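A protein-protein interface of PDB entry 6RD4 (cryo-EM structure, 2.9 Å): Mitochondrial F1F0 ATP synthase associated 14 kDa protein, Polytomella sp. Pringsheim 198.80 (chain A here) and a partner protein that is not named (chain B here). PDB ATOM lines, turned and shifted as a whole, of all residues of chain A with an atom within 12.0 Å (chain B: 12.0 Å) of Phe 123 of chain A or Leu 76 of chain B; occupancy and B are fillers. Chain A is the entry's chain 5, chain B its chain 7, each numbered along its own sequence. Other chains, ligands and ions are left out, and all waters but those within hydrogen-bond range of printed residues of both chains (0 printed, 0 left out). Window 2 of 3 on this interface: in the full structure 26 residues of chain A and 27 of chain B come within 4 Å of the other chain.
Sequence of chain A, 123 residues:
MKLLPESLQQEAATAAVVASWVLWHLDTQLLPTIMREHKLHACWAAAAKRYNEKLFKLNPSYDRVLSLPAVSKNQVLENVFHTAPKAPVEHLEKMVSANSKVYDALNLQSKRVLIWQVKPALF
The side-chain amide oxygen (OE1) of Gln 117 of chain A sits at hydrogen-bond distance from the guanidinium group (NH2) of Arg 81 of chain B (3.4 Å).
N of Val 79 of chain B sits at hydrogen-bond distance from O of Ala 121 of chain A, at 2.9 Å.
The backbone NH (N) of Phe 123 of chain A lies within hydrogen-bond range of the backbone carbonyl oxygen (O) of Ala 77 of chain B.
Among the printed residues, pairs that only touch across the chains: Pro 120 of chain A with Glu 78 of chain B, Pro 120 of chain A with Val 79 of chain B, Pro 120 of chain A with Ala 80 of chain B, Ala 121 of chain A with Ala 77 of chain B, Ala 121 of chain A with Glu 78 of chain B, Leu 122 of chain A with Leu 76 of chain B, Leu 122 of chain A with Glu 78 of chain B, Phe 123 of chain A with Leu 76 of chain B and Phe 123 of chain A with Val 79 of chain B.
Of chain B, only Leu 76 (3.4 Å), Ala 77 (3.2 Å) and Val 79 (3.6 Å) come within 4 Å of Phe 123 of chain A.
Leu 76 of chain B touches two residues of chain A.
Leu 122 of chain A touches two residues of chain B.
No residue of chain A comes within 4 Å of Ser 75 of chain B.
Val 79 of chain B touches just these residues of chain A: Pro 120, Ala 121 and Phe 123.
Of the printed residues of chain A, Glu 78 of chain B touches Pro 120, Ala 121 and Leu 122.
Printed residues of chain B within 4 Å of Gln 117 of chain A: Arg 81.
The nearest residue of chain B that does not touch Phe 123 of chain A is Ser 75 of chain B (4.8 Å).
The nearest residue of chain A that does not touch Leu 76 of chain B is Ala 121 of chain A (7.3 Å).
The nearest printed residue of chain B that does not touch Pro 120 of chain A is Val 84 of chain B (4.8 Å).
Hydrophobic or aromatic side chains of chain B that line the printed part of chain A: Leu 76, Val 79 and Ala 80.
Among the printed residues, no Asp or Glu carboxylate lies within 4 Å of a Lys or Arg side-chain nitrogen of the other chain.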
ATOM      1  N   ILE A 115      -7.524 -19.027  28.961  1.00  0.00           N
ATOM      2  CA  ILE A 115      -8.105 -19.300  27.656  1.00  0.00           C
ATOM      3  C   ILE A 115      -8.507 -18.023  26.941  1.00  0.00           C
ATOM      4  O   ILE A 115      -8.566 -17.997  25.714  1.00  0.00           O
ATOM      5  CB  ILE A 115      -9.276 -20.290  27.803  1.00  0.00           C
ATOM      6  CG1 ILE A 115      -9.686 -20.876  26.463  1.00  0.00           C
ATOM      7  CG2 ILE A 115     -10.455 -19.646  28.443  1.00  0.00           C
ATOM      8  CD1 ILE A 115      -8.609 -21.647  25.814  1.00  0.00           C
ATOM      9  N   TRP A 116      -8.725 -16.934  27.656  1.00  0.00           N
ATOM     10  CA  TRP A 116      -9.033 -15.677  27.007  1.00  0.00           C
ATOM     11  C   TRP A 116      -7.796 -14.847  26.807  1.00  0.00           C
ATOM     12  O   TRP A 116      -7.860 -13.801  26.171  1.00  0.00           O
ATOM     13  CB  TRP A 116     -10.060 -14.903  27.821  1.00  0.00           C
ATOM     14  CG  TRP A 116     -11.155 -15.761  28.274  1.00  0.00           C
ATOM     15  CD1 TRP A 116     -11.388 -16.167  29.532  1.00  0.00           C
ATOM     16  CD2 TRP A 116     -12.162 -16.354  27.465  1.00  0.00           C
ATOM     17  NE1 TRP A 116     -12.480 -16.974  29.573  1.00  0.00           N
ATOM     18  CE2 TRP A 116     -12.971 -17.109  28.307  1.00  0.00           C
ATOM     19  CE3 TRP A 116     -12.456 -16.319  26.104  1.00  0.00           C
ATOM     20  CZ2 TRP A 116     -14.057 -17.812  27.845  1.00  0.00           C
ATOM     21  CZ3 TRP A 116     -13.525 -17.023  25.650  1.00  0.00           C
ATOM     22  CH2 TRP A 116     -14.315 -17.760  26.511  1.00  0.00           C
ATOM     23  N   GLN A 117      -6.675 -15.292  27.343  1.00  0.00           N
ATOM     24  CA  GLN A 117      -5.420 -14.632  27.098  1.00  0.00           C
ATOM     25  C   GLN A 117      -4.636 -15.269  25.981  1.00  0.00           C
ATOM     26  O   GLN A 117      -3.817 -14.588  25.377  1.00  0.00           O
ATOM     27  CB  GLN A 117      -4.545 -14.654  28.339  1.00  0.00           C
ATOM     28  CG  GLN A 117      -5.238 -14.377  29.596  1.00  0.00           C
ATOM     29  CD  GLN A 117      -4.265 -14.196  30.699  1.00  0.00           C
ATOM     30  OE1 GLN A 117      -3.078 -14.088  30.464  1.00  0.00           O
ATOM     31  NE2 GLN A 117      -4.750 -14.174  31.917  1.00  0.00           N
ATOM     32  N   LYS A 119      -6.143 -17.501  23.482  1.00  0.00           N
ATOM     33  CA  LYS A 119      -6.994 -17.641  22.315  1.00  0.00           C
ATOM     34  C   LYS A 119      -8.063 -16.589  22.499  1.00  0.00           C
ATOM     35  O   LYS A 119      -9.105 -16.862  23.105  1.00  0.00           O
ATOM     36  CB  LYS A 119      -7.599 -19.033  22.222  1.00  0.00           C
ATOM     37  CG  LYS A 119      -6.675 -20.077  21.700  1.00  0.00           C
ATOM     38  CD  LYS A 119      -6.487 -19.930  20.230  1.00  0.00           C
ATOM     39  CE  LYS A 119      -5.504 -20.938  19.719  1.00  0.00           C
ATOM     40  NZ  LYS A 119      -5.199 -20.716  18.285  1.00  0.00           N
ATOM     41  N   PRO A 120      -7.832 -15.372  22.019  1.00  0.00           N
ATOM     42  CA  PRO A 120      -8.794 -14.301  22.244  1.00  0.00           C
ATOM     43  C   PRO A 120     -10.085 -14.534  21.483  1.00  0.00           C
ATOM     44  O   PRO A 120     -10.087 -15.025  20.355  1.00  0.00           O
ATOM     45  CB  PRO A 120      -8.059 -13.062  21.738  1.00  0.00           C
ATOM     46  CG  PRO A 120      -7.063 -13.556  20.848  1.00  0.00           C
ATOM     47  CD  PRO A 120      -6.630 -14.867  21.351  1.00  0.00           C
ATOM     48  N   ALA A 121     -11.186 -14.188  22.129  1.00  0.00           N
ATOM     49  CA  ALA A 121     -12.509 -14.543  21.657  1.00  0.00           C
ATOM     50  C   ALA A 121     -12.921 -13.679  20.485  1.00  0.00           C
ATOM     51  O   ALA A 121     -12.683 -12.475  20.481  1.00  0.00           O
ATOM     52  CB  ALA A 121     -13.514 -14.385  22.785  1.00  0.00           C
ATOM     53  N   LEU A 122     -13.561 -14.292  19.506  1.00  0.00           N
ATOM     54  CA  LEU A 122     -14.128 -13.562  18.388  1.00  0.00           C
ATOM     55  C   LEU A 122     -15.487 -13.017  18.778  1.00  0.00           C
ATOM     56  O   LEU A 122     -16.430 -13.780  18.975  1.00  0.00           O
ATOM     57  CB  LEU A 122     -14.260 -14.473  17.184  1.00  0.00           C
ATOM     58  CG  LEU A 122     -13.032 -14.529  16.325  1.00  0.00           C
ATOM     59  CD1 LEU A 122     -13.192 -15.571  15.288  1.00  0.00           C
ATOM     60  CD2 LEU A 122     -12.931 -13.221  15.688  1.00  0.00           C
ATOM     61  N   PHE A 123     -15.603 -11.709  18.872  1.00  0.00           N
ATOM     62  CA  PHE A 123     -16.878 -11.123  19.218  1.00  0.00           C
ATOM     63  C   PHE A 123     -17.546 -10.443  18.038  1.00  0.00           C
ATOM     64  O   PHE A 123     -16.894  -9.776  17.244  1.00  0.00           O
ATOM     65  CB  PHE A 123     -16.699 -10.137  20.354  1.00  0.00           C
ATOM     66  CG  PHE A 123     -16.838 -10.750  21.687  1.00  0.00           C
ATOM     67  CD1 PHE A 123     -18.070 -10.858  22.274  1.00  0.00           C
ATOM     68  CD2 PHE A 123     -15.747 -11.233  22.356  1.00  0.00           C
ATOM     69  CE1 PHE A 123     -18.205 -11.426  23.508  1.00  0.00           C
ATOM     70  CE2 PHE A 123     -15.876 -11.802  23.590  1.00  0.00           C
ATOM     71  CZ  PHE A 123     -17.107 -11.900  24.164  1.00  0.00           C
ATOM     72  N   LEU B  15     -14.998  -8.594   3.161  1.00  0.00           N
ATOM     73  CA  LEU B  15     -16.018  -8.861   2.169  1.00  0.00           C
ATOM     74  C   LEU B  15     -16.265  -7.643   1.316  1.00  0.00           C
ATOM     75  O   LEU B  15     -16.023  -6.524   1.742  1.00  0.00           O
ATOM     76  CB  LEU B  15     -17.308  -9.305   2.837  1.00  0.00           C
ATOM     77  CG  LEU B  15     -17.602 -10.787   2.738  1.00  0.00           C
ATOM     78  CD1 LEU B  15     -18.911 -11.052   3.382  1.00  0.00           C
ATOM     79  CD2 LEU B  15     -17.664 -11.179   1.291  1.00  0.00           C
ATOM     80  N   SER B  72     -25.359  -5.627   5.483  1.00  0.00           N
ATOM     81  CA  SER B  72     -24.616  -5.084   6.607  1.00  0.00           C
ATOM     82  C   SER B  72     -23.747  -6.195   7.171  1.00  0.00           C
ATOM     83  O   SER B  72     -24.264  -7.203   7.647  1.00  0.00           O
ATOM     84  CB  SER B  72     -25.559  -4.534   7.669  1.00  0.00           C
ATOM     85  OG  SER B  72     -26.581  -5.463   7.950  1.00  0.00           O
ATOM     86  N   LYS B  73     -22.438  -6.010   7.115  1.00  0.00           N
ATOM     87  CA  LYS B  73     -21.515  -7.082   7.433  1.00  0.00           C
ATOM     88  C   LYS B  73     -21.364  -7.246   8.937  1.00  0.00           C
ATOM     89  O   LYS B  73     -21.609  -6.317   9.709  1.00  0.00           O
ATOM     90  CB  LYS B  73     -20.157  -6.811   6.806  1.00  0.00           C
ATOM     91  CG  LYS B  73     -20.203  -6.538   5.328  1.00  0.00           C
ATOM     92  CD  LYS B  73     -20.272  -7.807   4.548  1.00  0.00           C
ATOM     93  CE  LYS B  73     -20.693  -7.542   3.125  1.00  0.00           C
ATOM     94  NZ  LYS B  73     -20.144  -6.270   2.634  1.00  0.00           N
ATOM     95  N   ILE B  74     -20.956  -8.441   9.355  1.00  0.00           N
ATOM     96  CA  ILE B  74     -20.733  -8.681  10.776  1.00  0.00           C
ATOM     97  C   ILE B  74     -19.406  -8.083  11.215  1.00  0.00           C
ATOM     98  O   ILE B  74     -19.361  -7.273  12.147  1.00  0.00           O
ATOM     99  CB  ILE B  74     -20.797 -10.181  11.103  1.00  0.00           C
ATOM    100  CG1 ILE B  74     -22.215 -10.700  10.937  1.00  0.00           C
ATOM    101  CG2 ILE B  74     -20.385 -10.404  12.527  1.00  0.00           C
ATOM    102  CD1 ILE B  74     -23.169 -10.133  11.935  1.00  0.00           C
ATOM    103  N   SER B  75     -18.320  -8.480  10.546  1.00  0.00           N
ATOM    104  CA  SER B  75     -16.955  -8.005  10.780  1.00  0.00           C
ATOM    105  C   SER B  75     -16.506  -8.289  12.214  1.00  0.00           C
ATOM    106  O   SER B  75     -16.398  -7.407  13.062  1.00  0.00           O
ATOM    107  CB  SER B  75     -16.793  -6.529  10.420  1.00  0.00           C
ATOM    108  OG  SER B  75     -15.443  -6.152  10.561  1.00  0.00           O
ATOM    109  N   LEU B  76     -16.305  -9.578  12.455  1.00  0.00           N
ATOM    110  CA  LEU B  76     -15.847 -10.073  13.740  1.00  0.00           C
ATOM    111  C   LEU B  76     -14.443  -9.589  14.037  1.00  0.00           C
ATOM    112  O   LEU B  76     -13.625  -9.396  13.139  1.00  0.00           O
ATOM    113  CB  LEU B  76     -15.866 -11.587  13.742  1.00  0.00           C
ATOM    114  CG  LEU B  76     -17.240 -12.178  13.599  1.00  0.00           C
ATOM    115  CD1 LEU B  76     -17.056 -13.608  13.399  1.00  0.00           C
ATOM    116  CD2 LEU B  76     -17.962 -11.919  14.862  1.00  0.00           C
ATOM    117  N   ALA B  77     -14.165  -9.394  15.317  1.00  0.00           N
ATOM    118  CA  ALA B  77     -12.854  -8.937  15.721  1.00  0.00           C
ATOM    119  C   ALA B  77     -12.577  -9.438  17.115  1.00  0.00           C
ATOM    120  O   ALA B  77     -13.481  -9.561  17.936  1.00  0.00           O
ATOM    121  CB  ALA B  77     -12.741  -7.425  15.686  1.00  0.00           C
ATOM    122  N   GLU B  78     -11.310  -9.700  17.376  1.00  0.00           N
ATOM    123  CA  GLU B  78     -10.906 -10.448  18.543  1.00  0.00           C
ATOM    124  C   GLU B  78     -10.730  -9.518  19.724  1.00  0.00           C
ATOM    125  O   GLU B  78     -10.084  -8.477  19.610  1.00  0.00           O
ATOM    126  CB  GLU B  78      -9.616 -11.195  18.253  1.00  0.00           C
ATOM    127  CG  GLU B  78      -9.732 -12.013  17.012  1.00  0.00           C
ATOM    128  CD  GLU B  78      -8.589 -12.947  16.827  1.00  0.00           C
ATOM    129  OE1 GLU B  78      -7.683 -12.932  17.666  1.00  0.00           O
ATOM    130  OE2 GLU B  78      -8.584 -13.706  15.844  1.00  0.00           O
ATOM    131  N   VAL B  79     -11.313  -9.896  20.850  1.00  0.00           N
ATOM    132  CA  VAL B  79     -11.128  -9.179  22.098  1.00  0.00           C
ATOM    133  C   VAL B  79      -9.984  -9.857  22.828  1.00  0.00           C
ATOM    134  O   VAL B  79     -10.131 -10.967  23.333  1.00  0.00           O
ATOM    135  CB  VAL B  79     -12.405  -9.183  22.935  1.00  0.00           C
ATOM    136  CG1 VAL B  79     -12.140  -8.563  24.262  1.00  0.00           C
ATOM    137  CG2 VAL B  79     -13.465  -8.438  22.213  1.00  0.00           C
ATOM    138  N   ALA B  80      -8.841  -9.202  22.872  1.00  0.00           N
ATOM    139  CA  ALA B  80      -7.650  -9.787  23.446  1.00  0.00           C
ATOM    140  C   ALA B  80      -7.333  -9.108  24.759  1.00  0.00           C
ATOM    141  O   ALA B  80      -7.783  -7.996  25.023  1.00  0.00           O
ATOM    142  CB  ALA B  80      -6.478  -9.661  22.488  1.00  0.00           C
ATOM    143  N   ARG B  81      -6.579  -9.805  25.601  1.00  0.00           N
ATOM    144  CA  ARG B  81      -6.216  -9.226  26.882  1.00  0.00           C
ATOM    145  C   ARG B  81      -5.250  -8.083  26.689  1.00  0.00           C
ATOM    146  O   ARG B  81      -5.436  -7.000  27.243  1.00  0.00           O
ATOM    147  CB  ARG B  81      -5.608 -10.273  27.796  1.00  0.00           C
ATOM    148  CG  ARG B  81      -5.089  -9.685  29.057  1.00  0.00           C
ATOM    149  CD  ARG B  81      -4.865 -10.718  30.080  1.00  0.00           C
ATOM    150  NE  ARG B  81      -4.273 -10.154  31.277  1.00  0.00           N
ATOM    151  CZ  ARG B  81      -2.980 -10.201  31.541  1.00  0.00           C
ATOM    152  NH1 ARG B  81      -2.507  -9.679  32.652  1.00  0.00           N
ATOM    153  NH2 ARG B  81      -2.162 -10.776  30.684  1.00  0.00           N
ATOM    154  N   VAL B  84      -3.648  -9.090  19.844  1.00  0.00           N
ATOM    155  CA  VAL B  84      -3.718 -10.346  19.120  1.00  0.00           C
ATOM    156  C   VAL B  84      -2.330 -10.881  18.847  1.00  0.00           C
ATOM    157  O   VAL B  84      -2.129 -12.093  18.785  1.00  0.00           O
ATOM    158  CB  VAL B  84      -4.518 -10.143  17.833  1.00  0.00           C
ATOM    159  CG1 VAL B  84      -4.799 -11.421  17.182  1.00  0.00           C
ATOM    160  CG2 VAL B  84      -5.803  -9.515  18.167  1.00  0.00           C
